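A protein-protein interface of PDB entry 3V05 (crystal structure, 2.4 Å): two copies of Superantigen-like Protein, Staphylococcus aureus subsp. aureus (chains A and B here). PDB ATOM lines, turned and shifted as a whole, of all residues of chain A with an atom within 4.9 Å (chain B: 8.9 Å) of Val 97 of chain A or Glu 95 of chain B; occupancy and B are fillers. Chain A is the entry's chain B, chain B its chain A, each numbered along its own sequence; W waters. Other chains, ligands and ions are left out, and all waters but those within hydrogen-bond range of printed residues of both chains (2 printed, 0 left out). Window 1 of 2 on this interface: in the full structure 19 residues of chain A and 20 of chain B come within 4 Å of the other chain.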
ATOM      1  N   ASP A  54     -20.194  -7.980  18.908  1.00  0.00           N
ATOM      2  CA  ASP A  54     -19.365  -6.952  19.537  1.00  0.00           C
ATOM      3  C   ASP A  54     -19.215  -5.712  18.638  1.00  0.00           C
ATOM      4  O   ASP A  54     -19.452  -5.773  17.430  1.00  0.00           O
ATOM      5  CB  ASP A  54     -18.018  -7.513  20.023  1.00  0.00           C
ATOM      6  CG  ASP A  54     -17.109  -7.957  18.908  1.00  0.00           C
ATOM      7  OD1 ASP A  54     -17.199  -7.395  17.801  1.00  0.00           O
ATOM      8  OD2 ASP A  54     -16.265  -8.852  19.169  1.00  0.00           O
ATOM      9  N   LYS A  55     -18.830  -4.592  19.246  1.00  0.00           N
ATOM     10  CA  LYS A  55     -18.724  -3.317  18.540  1.00  0.00           C
ATOM     11  C   LYS A  55     -17.290  -2.824  18.388  1.00  0.00           C
ATOM     12  O   LYS A  55     -16.988  -1.663  18.668  1.00  0.00           O
ATOM     13  CB  LYS A  55     -19.572  -2.263  19.264  1.00  0.00           C
ATOM     14  CG  LYS A  55     -21.057  -2.549  19.220  1.00  0.00           C
ATOM     15  CD  LYS A  55     -21.844  -1.529  20.013  1.00  0.00           C
ATOM     16  CE  LYS A  55     -23.342  -1.676  19.791  1.00  0.00           C
ATOM     17  NZ  LYS A  55     -23.861  -3.024  20.123  1.00  0.00           N
ATOM     18  N   GLY A  56     -16.411  -3.705  17.931  1.00  0.00           N
ATOM     19  CA  GLY A  56     -15.020  -3.338  17.726  1.00  0.00           C
ATOM     20  C   GLY A  56     -14.157  -4.463  17.203  1.00  0.00           C
ATOM     21  O   GLY A  56     -14.616  -5.599  17.068  1.00  0.00           O
ATOM     22  N   PHE A  67      -7.739  -2.277  21.078  1.00  0.00           N
ATOM     23  CA  PHE A  67      -9.090  -2.624  20.720  1.00  0.00           C
ATOM     24  C   PHE A  67      -9.648  -1.358  20.100  1.00  0.00           C
ATOM     25  O   PHE A  67      -9.560  -0.282  20.693  1.00  0.00           O
ATOM     26  CB  PHE A  67      -9.909  -3.098  21.917  1.00  0.00           C
ATOM     27  CG  PHE A  67     -11.269  -3.597  21.541  1.00  0.00           C
ATOM     28  CD1 PHE A  67     -11.424  -4.849  20.993  1.00  0.00           C
ATOM     29  CD2 PHE A  67     -12.394  -2.799  21.712  1.00  0.00           C
ATOM     30  CE1 PHE A  67     -12.683  -5.322  20.633  1.00  0.00           C
ATOM     31  CE2 PHE A  67     -13.655  -3.258  21.351  1.00  0.00           C
ATOM     32  CZ  PHE A  67     -13.798  -4.523  20.814  1.00  0.00           C
ATOM     33  N   GLU A  95     -11.088   5.298  28.401  1.00  0.00           N
ATOM     34  CA  GLU A  95     -11.586   3.986  28.800  1.00  0.00           C
ATOM     35  C   GLU A  95     -10.646   2.856  28.461  1.00  0.00           C
ATOM     36  O   GLU A  95      -9.966   2.880  27.445  1.00  0.00           O
ATOM     37  CB  GLU A  95     -12.918   3.651  28.113  1.00  0.00           C
ATOM     38  CG  GLU A  95     -14.087   4.515  28.505  1.00  0.00           C
ATOM     39  CD  GLU A  95     -13.955   5.923  27.991  1.00  0.00           C
ATOM     40  OE1 GLU A  95     -14.238   6.857  28.759  1.00  0.00           O
ATOM     41  OE2 GLU A  95     -13.537   6.091  26.828  1.00  0.00           O
ATOM     42  N   THR A  96     -10.632   1.858  29.336  1.00  0.00           N
ATOM     43  CA  THR A  96      -9.920   0.622  29.101  1.00  0.00           C
ATOM     44  C   THR A  96     -11.049  -0.269  28.612  1.00  0.00           C
ATOM     45  O   THR A  96     -12.069  -0.368  29.279  1.00  0.00           O
ATOM     46  CB  THR A  96      -9.273   0.079  30.388  1.00  0.00           C
ATOM     47  OG1 THR A  96      -8.186   0.934  30.751  1.00  0.00           O
ATOM     48  CG2 THR A  96      -8.728  -1.320  30.190  1.00  0.00           C
ATOM     49  N   VAL A  97     -10.893  -0.861  27.429  1.00  0.00           N
ATOM     50  CA  VAL A  97     -11.912  -1.728  26.835  1.00  0.00           C
ATOM     51  C   VAL A  97     -11.317  -3.112  26.589  1.00  0.00           C
ATOM     52  O   VAL A  97     -10.252  -3.237  25.987  1.00  0.00           O
ATOM     53  CB  VAL A  97     -12.442  -1.150  25.500  1.00  0.00           C
ATOM     54  CG1 VAL A  97     -13.464  -2.098  24.861  1.00  0.00           C
ATOM     55  CG2 VAL A  97     -13.046   0.226  25.714  1.00  0.00           C
ATOM     56  N   ASN A  98     -12.001  -4.148  27.067  1.00  0.00           N
ATOM     57  CA  ASN A  98     -11.506  -5.523  26.938  1.00  0.00           C
ATOM     58  C   ASN A  98     -10.044  -5.673  27.365  1.00  0.00           C
ATOM     59  O   ASN A  98      -9.283  -6.424  26.759  1.00  0.00           O
ATOM     60  CB  ASN A  98     -11.718  -6.049  25.513  1.00  0.00           C
ATOM     61  CG  ASN A  98     -13.175  -6.287  25.197  1.00  0.00           C
ATOM     62  OD1 ASN A  98     -14.002  -6.360  26.098  1.00  0.00           O
ATOM     63  ND2 ASN A  98     -13.497  -6.431  23.914  1.00  0.00           N
ATOM     64  N   GLY A  99      -9.666  -4.952  28.417  1.00  0.00           N
ATOM     65  CA  GLY A  99      -8.308  -5.012  28.960  1.00  0.00           C
ATOM     66  C   GLY A  99      -7.234  -4.287  28.162  1.00  0.00           C
ATOM     67  O   GLY A  99      -6.083  -4.266  28.571  1.00  0.00           O
ATOM     68  N   ARG A 100      -7.618  -3.684  27.040  1.00  0.00           N
ATOM     69  CA  ARG A 100      -6.694  -2.967  26.160  1.00  0.00           C
ATOM     70  C   ARG A 100      -6.948  -1.468  26.076  1.00  0.00           C
ATOM     71  O   ARG A 100      -8.012  -0.961  26.451  1.00  0.00           O
ATOM     72  CB  ARG A 100      -6.838  -3.459  24.709  1.00  0.00           C
ATOM     73  CG  ARG A 100      -6.180  -4.773  24.326  1.00  0.00           C
ATOM     74  CD  ARG A 100      -6.880  -5.981  24.842  1.00  0.00           C
ATOM     75  NE  ARG A 100      -6.399  -7.177  24.145  1.00  0.00           N
ATOM     76  CZ  ARG A 100      -6.791  -8.416  24.416  1.00  0.00           C
ATOM     77  NH1 ARG A 100      -6.301  -9.431  23.716  1.00  0.00           N
ATOM     78  NH2 ARG A 100      -7.668  -8.643  25.385  1.00  0.00           N
ATOM     79  N   TYR A 102      -7.806   1.745  24.073  1.00  0.00           N
ATOM     80  CA  TYR A 102      -8.905   1.847  23.141  1.00  0.00           C
ATOM     81  C   TYR A 102      -8.911   3.128  22.329  1.00  0.00           C
ATOM     82  O   TYR A 102      -8.528   4.187  22.813  1.00  0.00           O
ATOM     83  CB  TYR A 102     -10.168   1.751  23.995  1.00  0.00           C
ATOM     84  CG  TYR A 102     -11.504   1.804  23.311  1.00  0.00           C
ATOM     85  CD1 TYR A 102     -11.983   0.717  22.593  1.00  0.00           C
ATOM     86  CD2 TYR A 102     -12.338   2.899  23.463  1.00  0.00           C
ATOM     87  CE1 TYR A 102     -13.226   0.742  21.993  1.00  0.00           C
ATOM     88  CE2 TYR A 102     -13.595   2.932  22.876  1.00  0.00           C
ATOM     89  CZ  TYR A 102     -14.034   1.852  22.144  1.00  0.00           C
ATOM     90  OH  TYR A 102     -15.277   1.876  21.558  1.00  0.00           O
ATOM     91  N   TYR B  33     -28.475 -10.073  19.739  1.00  0.00           N
ATOM     92  CA  TYR B  33     -28.525  -8.795  20.442  1.00  0.00           C
ATOM     93  C   TYR B  33     -29.884  -8.522  21.082  1.00  0.00           C
ATOM     94  O   TYR B  33     -29.960  -8.205  22.264  1.00  0.00           O
ATOM     95  CB  TYR B  33     -28.123  -7.644  19.518  1.00  0.00           C
ATOM     96  CG  TYR B  33     -28.002  -6.338  20.250  1.00  0.00           C
ATOM     97  CD1 TYR B  33     -29.036  -5.410  20.234  1.00  0.00           C
ATOM     98  CD2 TYR B  33     -26.862  -6.043  20.990  1.00  0.00           C
ATOM     99  CE1 TYR B  33     -28.925  -4.215  20.917  1.00  0.00           C
ATOM    100  CE2 TYR B  33     -26.746  -4.863  21.670  1.00  0.00           C
ATOM    101  CZ  TYR B  33     -27.782  -3.948  21.634  1.00  0.00           C
ATOM    102  OH  TYR B  33     -27.657  -2.768  22.315  1.00  0.00           O
ATOM    103  N   LYS B  36     -30.922 -10.517  24.233  1.00  0.00           N
ATOM    104  CA  LYS B  36     -30.274 -10.157  25.486  1.00  0.00           C
ATOM    105  C   LYS B  36     -31.261  -9.647  26.526  1.00  0.00           C
ATOM    106  O   LYS B  36     -32.295  -9.078  26.193  1.00  0.00           O
ATOM    107  CB  LYS B  36     -29.214  -9.064  25.273  1.00  0.00           C
ATOM    108  CG  LYS B  36     -27.949  -9.475  24.519  1.00  0.00           C
ATOM    109  CD  LYS B  36     -27.089  -8.237  24.319  1.00  0.00           C
ATOM    110  CE  LYS B  36     -25.796  -8.500  23.556  1.00  0.00           C
ATOM    111  NZ  LYS B  36     -24.749  -9.196  24.336  1.00  0.00           N
ATOM    112  N   PHE B  67     -20.856   0.728  33.811  1.00  0.00           N
ATOM    113  CA  PHE B  67     -20.320   1.898  33.145  1.00  0.00           C
ATOM    114  C   PHE B  67     -21.172   2.055  31.892  1.00  0.00           C
ATOM    115  O   PHE B  67     -21.374   1.092  31.150  1.00  0.00           O
ATOM    116  CB  PHE B  67     -18.840   1.738  32.837  1.00  0.00           C
ATOM    117  CG  PHE B  67     -18.209   2.973  32.248  1.00  0.00           C
ATOM    118  CD1 PHE B  67     -17.788   4.011  33.065  1.00  0.00           C
ATOM    119  CD2 PHE B  67     -18.027   3.091  30.879  1.00  0.00           C
ATOM    120  CE1 PHE B  67     -17.202   5.151  32.526  1.00  0.00           C
ATOM    121  CE2 PHE B  67     -17.446   4.229  30.336  1.00  0.00           C
ATOM    122  CZ  PHE B  67     -17.032   5.256  31.163  1.00  0.00           C
ATOM    123  N   LEU B  71     -22.097   8.182  23.801  1.00  0.00           N
ATOM    124  CA  LEU B  71     -21.584   8.270  22.420  1.00  0.00           C
ATOM    125  C   LEU B  71     -22.429   9.109  21.466  1.00  0.00           C
ATOM    126  O   LEU B  71     -22.262   9.029  20.256  1.00  0.00           O
ATOM    127  CB  LEU B  71     -21.438   6.849  21.846  1.00  0.00           C
ATOM    128  CG  LEU B  71     -20.610   5.884  22.707  1.00  0.00           C
ATOM    129  CD1 LEU B  71     -20.563   4.486  22.088  1.00  0.00           C
ATOM    130  CD2 LEU B  71     -19.215   6.436  22.906  1.00  0.00           C
ATOM    131  N   VAL B  91     -28.433  -2.551  28.569  1.00  0.00           N
ATOM    132  CA  VAL B  91     -28.328  -3.695  27.710  1.00  0.00           C
ATOM    133  C   VAL B  91     -26.822  -3.895  27.731  1.00  0.00           C
ATOM    134  O   VAL B  91     -26.061  -3.052  27.236  1.00  0.00           O
ATOM    135  CB  VAL B  91     -28.884  -3.460  26.297  1.00  0.00           C
ATOM    136  CG1 VAL B  91     -28.624  -4.685  25.417  1.00  0.00           C
ATOM    137  CG2 VAL B  91     -30.390  -3.159  26.355  1.00  0.00           C
ATOM    138  N   ILE B  92     -26.394  -4.983  28.354  1.00  0.00           N
ATOM    139  CA  ILE B  92     -24.967  -5.251  28.532  1.00  0.00           C
ATOM    140  C   ILE B  92     -24.318  -5.720  27.235  1.00  0.00           C
ATOM    141  O   ILE B  92     -24.651  -6.769  26.696  1.00  0.00           O
ATOM    142  CB  ILE B  92     -24.713  -6.273  29.670  1.00  0.00           C
ATOM    143  CG1 ILE B  92     -25.429  -5.823  30.944  1.00  0.00           C
ATOM    144  CG2 ILE B  92     -23.196  -6.446  29.931  1.00  0.00           C
ATOM    145  CD1 ILE B  92     -25.106  -4.357  31.349  1.00  0.00           C
ATOM    146  N   GLU B  93     -23.391  -4.908  26.746  1.00  0.00           N
ATOM    147  CA  GLU B  93     -22.661  -5.176  25.508  1.00  0.00           C
ATOM    148  C   GLU B  93     -21.600  -6.248  25.744  1.00  0.00           C
ATOM    149  O   GLU B  93     -21.354  -6.651  26.889  1.00  0.00           O
ATOM    150  CB  GLU B  93     -21.991  -3.873  25.034  1.00  0.00           C
ATOM    151  CG  GLU B  93     -22.970  -2.715  24.724  1.00  0.00           C
ATOM    152  CD  GLU B  93     -23.823  -2.975  23.489  1.00  0.00           C
ATOM    153  OE1 GLU B  93     -23.420  -3.832  22.671  1.00  0.00           O
ATOM    154  OE2 GLU B  93     -24.886  -2.318  23.325  1.00  0.00           O
ATOM    155  N   GLU B  94     -20.957  -6.698  24.674  1.00  0.00           N
ATOM    156  CA  GLU B  94     -19.905  -7.718  24.790  1.00  0.00           C
ATOM    157  C   GLU B  94     -18.613  -7.171  25.393  1.00  0.00           C
ATOM    158  O   GLU B  94     -17.843  -7.923  25.990  1.00  0.00           O
ATOM    159  CB  GLU B  94     -19.584  -8.330  23.420  1.00  0.00           C
ATOM    160  CG  GLU B  94     -20.744  -9.060  22.809  1.00  0.00           C
ATOM    161  CD  GLU B  94     -21.268 -10.151  23.714  1.00  0.00           C
ATOM    162  OE1 GLU B  94     -22.505 -10.272  23.817  1.00  0.00           O
ATOM    163  OE2 GLU B  94     -20.450 -10.863  24.347  1.00  0.00           O
ATOM    164  N   GLU B  95     -18.379  -5.870  25.230  1.00  0.00           N
ATOM    165  CA  GLU B  95     -17.160  -5.244  25.723  1.00  0.00           C
ATOM    166  C   GLU B  95     -17.162  -5.027  27.224  1.00  0.00           C
ATOM    167  O   GLU B  95     -18.166  -4.614  27.798  1.00  0.00           O
ATOM    168  CB  GLU B  95     -16.936  -3.854  25.081  1.00  0.00           C
ATOM    169  CG  GLU B  95     -16.615  -3.840  23.590  1.00  0.00           C
ATOM    170  CD  GLU B  95     -17.783  -4.241  22.713  1.00  0.00           C
ATOM    171  OE1 GLU B  95     -17.551  -4.988  21.739  1.00  0.00           O
ATOM    172  OE2 GLU B  95     -18.933  -3.831  23.002  1.00  0.00           O
ATOM    173  N   THR B  96     -16.029  -5.301  27.853  1.00  0.00           N
ATOM    174  CA  THR B  96     -15.844  -4.968  29.249  1.00  0.00           C
ATOM    175  C   THR B  96     -15.221  -3.568  29.165  1.00  0.00           C
ATOM    176  O   THR B  96     -14.324  -3.339  28.352  1.00  0.00           O
ATOM    177  CB  THR B  96     -14.895  -5.930  29.965  1.00  0.00           C
ATOM    178  OG1 THR B  96     -15.419  -7.265  29.917  1.00  0.00           O
ATOM    179  CG2 THR B  96     -14.731  -5.525  31.415  1.00  0.00           C
ATOM    180  N   VAL B  97     -15.699  -2.625  29.966  1.00  0.00           N
ATOM    181  CA  VAL B  97     -15.154  -1.267  29.931  1.00  0.00           C
ATOM    182  C   VAL B  97     -14.835  -0.810  31.343  1.00  0.00           C
ATOM    183  O   VAL B  97     -15.700  -0.820  32.212  1.00  0.00           O
ATOM    184  CB  VAL B  97     -16.134  -0.274  29.250  1.00  0.00           C
ATOM    185  CG1 VAL B  97     -15.538   1.124  29.212  1.00  0.00           C
ATOM    186  CG2 VAL B  97     -16.472  -0.740  27.828  1.00  0.00           C
ATOM    187  N   ASN B  98     -13.588  -0.412  31.567  1.00  0.00           N
ATOM    188  CA  ASN B  98     -13.130   0.014  32.886  1.00  0.00           C
ATOM    189  C   ASN B  98     -13.414  -1.065  33.932  1.00  0.00           C
ATOM    190  O   ASN B  98     -13.783  -0.764  35.077  1.00  0.00           O
ATOM    191  CB  ASN B  98     -13.772   1.350  33.293  1.00  0.00           C
ATOM    192  CG  ASN B  98     -13.310   2.510  32.437  1.00  0.00           C
ATOM    193  OD1 ASN B  98     -12.241   2.466  31.826  1.00  0.00           O
ATOM    194  ND2 ASN B  98     -14.107   3.571  32.408  1.00  0.00           N
ATOM    195  N   GLY B  99     -13.247  -2.319  33.518  1.00  0.00           N
ATOM    196  CA  GLY B  99     -13.455  -3.472  34.384  1.00  0.00           C
ATOM    197  C   GLY B  99     -14.898  -3.728  34.790  1.00  0.00           C
ATOM    198  O   GLY B  99     -15.155  -4.466  35.734  1.00  0.00           O
ATOM    199  N   ARG B 100     -15.843  -3.147  34.062  1.00  0.00           N
ATOM    200  CA  ARG B 100     -17.256  -3.294  34.389  1.00  0.00           C
ATOM    201  C   ARG B 100     -18.109  -3.683  33.194  1.00  0.00           C
ATOM    202  O   ARG B 100     -17.677  -3.602  32.041  1.00  0.00           O
ATOM    203  CB  ARG B 100     -17.781  -1.969  34.956  1.00  0.00           C
ATOM    204  CG  ARG B 100     -17.165  -1.594  36.285  1.00  0.00           C
ATOM    205  CD  ARG B 100     -17.366  -0.144  36.615  1.00  0.00           C
ATOM    206  NE  ARG B 100     -16.927   0.179  37.977  1.00  0.00           N
ATOM    207  CZ  ARG B 100     -15.660   0.346  38.354  1.00  0.00           C
ATOM    208  NH1 ARG B 100     -15.385   0.653  39.617  1.00  0.00           N
ATOM    209  NH2 ARG B 100     -14.661   0.201  37.484  1.00  0.00           N
ATOM    210  N   GLN B 101     -19.325  -4.128  33.503  1.00  0.00           N
ATOM    211  CA  GLN B 101     -20.318  -4.447  32.505  1.00  0.00           C
ATOM    212  C   GLN B 101     -20.653  -3.100  31.865  1.00  0.00           C
ATOM    213  O   GLN B 101     -20.781  -2.095  32.561  1.00  0.00           O
ATOM    214  CB  GLN B 101     -21.537  -5.106  33.139  1.00  0.00           C
ATOM    215  CG  GLN B 101     -21.343  -6.583  33.494  1.00  0.00           C
ATOM    216  CD  GLN B 101     -22.514  -7.148  34.291  1.00  0.00           C
ATOM    217  OE1 GLN B 101     -22.744  -6.763  35.435  1.00  0.00           O
ATOM    218  NE2 GLN B 101     -23.227  -8.086  33.704  1.00  0.00           N
ATOM    219  N   TYR B 102     -20.777  -3.100  30.544  1.00  0.00           N
ATOM    220  CA  TYR B 102     -20.965  -1.895  29.766  1.00  0.00           C
ATOM    221  C   TYR B 102     -22.264  -1.862  28.999  1.00  0.00           C
ATOM    222  O   TYR B 102     -22.704  -2.867  28.465  1.00  0.00           O
ATOM    223  CB  TYR B 102     -19.802  -1.821  28.768  1.00  0.00           C
ATOM    224  CG  TYR B 102     -19.732  -0.596  27.875  1.00  0.00           C
ATOM    225  CD1 TYR B 102     -19.525   0.657  28.417  1.00  0.00           C
ATOM    226  CD2 TYR B 102     -19.785  -0.707  26.481  1.00  0.00           C
ATOM    227  CE1 TYR B 102     -19.418   1.781  27.616  1.00  0.00           C
ATOM    228  CE2 TYR B 102     -19.680   0.418  25.669  1.00  0.00           C
ATOM    229  CZ  TYR B 102     -19.496   1.665  26.253  1.00  0.00           C
ATOM    230  OH  TYR B 102     -19.386   2.810  25.490  1.00  0.00           O
ATOM    231  N   SER B 103     -22.859  -0.680  28.937  1.00  0.00           N
ATOM    232  CA  SER B 103     -24.084  -0.445  28.188  1.00  0.00           C
ATOM    233  C   SER B 103     -23.930   0.936  27.570  1.00  0.00           C
ATOM    234  O   SER B 103     -23.200   1.779  28.107  1.00  0.00           O
ATOM    235  CB  SER B 103     -25.303  -0.512  29.108  1.00  0.00           C
ATOM    236  OG  SER B 103     -26.510  -0.293  28.399  1.00  0.00           O
ATOM    237  N   ILE B 104     -24.621   1.179  26.465  1.00  0.00           N
ATOM    238  CA  ILE B 104     -24.519   2.452  25.743  1.00  0.00           C
ATOM    239  C   ILE B 104     -25.811   3.251  25.808  1.00  0.00           C
ATOM    240  O   ILE B 104     -26.870   2.745  25.430  1.00  0.00           O
ATOM    241  CB  ILE B 104     -24.175   2.216  24.248  1.00  0.00           C
ATOM    242  CG1 ILE B 104     -22.900   1.379  24.122  1.00  0.00           C
ATOM    243  CG2 ILE B 104     -24.030   3.548  23.514  1.00  0.00           C
ATOM    244  CD1 ILE B 104     -22.500   1.040  22.686  1.00  0.00           C
ATOM    245  N   LYS B 193     -29.289  -2.994  13.960  1.00  0.00           N
ATOM    246  CA  LYS B 193     -29.386  -2.577  15.357  1.00  0.00           C
ATOM    247  C   LYS B 193     -29.542  -1.063  15.415  1.00  0.00           C
ATOM    248  O   LYS B 193     -29.215  -0.368  14.460  1.00  0.00           O
ATOM    249  CB  LYS B 193     -28.130  -2.985  16.130  1.00  0.00           C
ATOM    250  CG  LYS B 193     -27.836  -4.500  16.178  1.00  0.00           C
ATOM    251  CD  LYS B 193     -26.485  -4.797  16.875  1.00  0.00           C
ATOM    252  CE  LYS B 193     -25.295  -4.178  16.118  1.00  0.00           C
ATOM    253  NZ  LYS B 193     -23.955  -4.426  16.767  1.00  0.00           N
HETATM  254  O   HOH W   1     -13.208   5.999  31.230  1.00  0.00           O
HETATM  255  O   HOH W   2     -15.898  -7.168  22.914  1.00  0.00           O
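The side-chain amino group (NZ) of Lys 36 of chain B lies within salt-bridge range of the side-chain carboxylate (OE1) of Glu 94 of chain B (2.5 Å). O of Asn 98 of chain A is in hydrogen-bond range of NH2 of Arg 100 of chain A (3.1 Å). N of Glu 93 of chain B lies within hydrogen-bond range of O of Tyr 102 of chain B, 2.8 Å away. N of Phe 67 of chain B is in hydrogen-bond range of O of Gln 101 of chain B, at 3.1 Å. The backbone carbonyl oxygen (O) of Phe 67 of chain B is in hydrogen-bond range of the backbone NH (N) of Ser 103 of chain B (3.2 Å). The side-chain carboxylate of Glu 93 of chain B lies within hydrogen-bond range of the side-chain hydroxyl of Tyr 33 of chain B (3.0 Å).
Val 97 of chain A touches just these residues of chain B: Glu 95 (3.8 Å) and Thr 96 (3.3 Å). Of chain A, only Asp 54 (3.1 Å), Lys 55 (2.8 Å), Phe 67 (3.8 Å), Val 97 (3.8 Å) and Asn 98 (3.4 Å) come within 4 Å of Glu 95 of chain B. Asn 98 of chain A touches just these residues of chain B: Glu 95 and Thr 96. Of the printed residues of chain A, Val 97 of chain B touches Glu 95 and Thr 96. Of the printed residues of chain B, Glu 95 of chain A touches Phe 67 (3.8 Å), Val 97 (3.8 Å) and Asn 98 (3.4 Å). Of the printed residues of chain A, Lys 193 of chain B touches Lys 55 (3.6 Å). Of the printed residues of chain A, Glu 94 of chain B touches Asp 54 (3.8 Å). Ser 103 of chain B touches none of the printed residues of chain A. The nearest residue of chain B that does not touch Val 97 of chain A is Val 97 of chain B (4.1 Å).
Phe 67 of chain A touches Glu 95 of chain B, and with the chains exchanged Glu 95 of chain A touches Phe 67 of chain B. Glu 95 of chain A touches Val 97 of chain B, and with the chains exchanged Val 97 of chain A touches Glu 95 of chain B. Glu 95 of chain A touches Asn 98 of chain B, and with the chains exchanged Asn 98 of chain A touches Glu 95 of chain B. Thr 96 of chain A touches Asn 98 of chain B, and with the chains exchanged Asn 98 of chain A touches Thr 96 of chain B.
Among the printed residues, merely in contact across the chains: Asp 54 of chain A with Glu 95 of chain B, Val 97 of chain A with Thr 96 of chain B, Thr 96 of chain A with Val 97 of chain B, Asn 98 of chain A with Glu 95 of chain B, Glu 95 of chain A with Asn 98 of chain B, Lys 55 of chain A with Lys 193 of chain B, Lys 55 of chain A with Tyr 33 of chain B, Glu 95 of chain A with Val 97 of chain B, Phe 67 of chain A with Glu 95 of chain B, Lys 55 of chain A with Ile 104 of chain B, Val 97 of chain A with Glu 95 of chain B, Asp 54 of chain A with Glu 94 of chain B, Glu 95 of chain A with Phe 67 of chain B and Thr 96 of chain A with Thr 96 of chain B.
Water W2 bridges ND2 of Asn 98 of chain A (2.7 Å) and OE1 of Glu 95 of chain B (3.0 Å). Water W1 bridges OE1 of Glu 95 of chain A and ND2 of Asn 98 of chain B.
The backbone NH (N) of Asn 98 of chain B lies within hydrogen-bond range of the backbone carbonyl oxygen (O) of Thr 96 of chain A (2.7 Å). The side-chain amino group (NZ) of Lys 55 of chain A is in salt-bridge range of the side-chain carboxylate (OE1) of Glu 93 of chain B (2.7 Å). O of Thr 96 of chain B sits at hydrogen-bond distance from N of Asn 98 of chain A. The backbone NH of Lys 55 of chain A is in hydrogen-bond range of the side-chain carboxylate of Glu 95 of chain B (2.8 Å).
Of the 11 printed residues of chain A, 7 touch a printed residue of chain B. Printed residues of chain A that touch a printed residue of chain B: Asp 54, Lys 55, Phe 67, Glu 95, Thr 96, Val 97 and Asn 98. Printed residues of chain B that touch a printed residue of chain A: Tyr 33, Phe 67, Glu 93, Glu 94, Glu 95, Thr 96, Val 97, Asn 98, Ile 104 and Lys 193. Hydrophobic or aromatic side chains of chain B that line the printed part of chain A: Tyr 33, Phe 67, Val 97 and Ile 104. Among the printed residues, 18 pairs touch across the chains.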
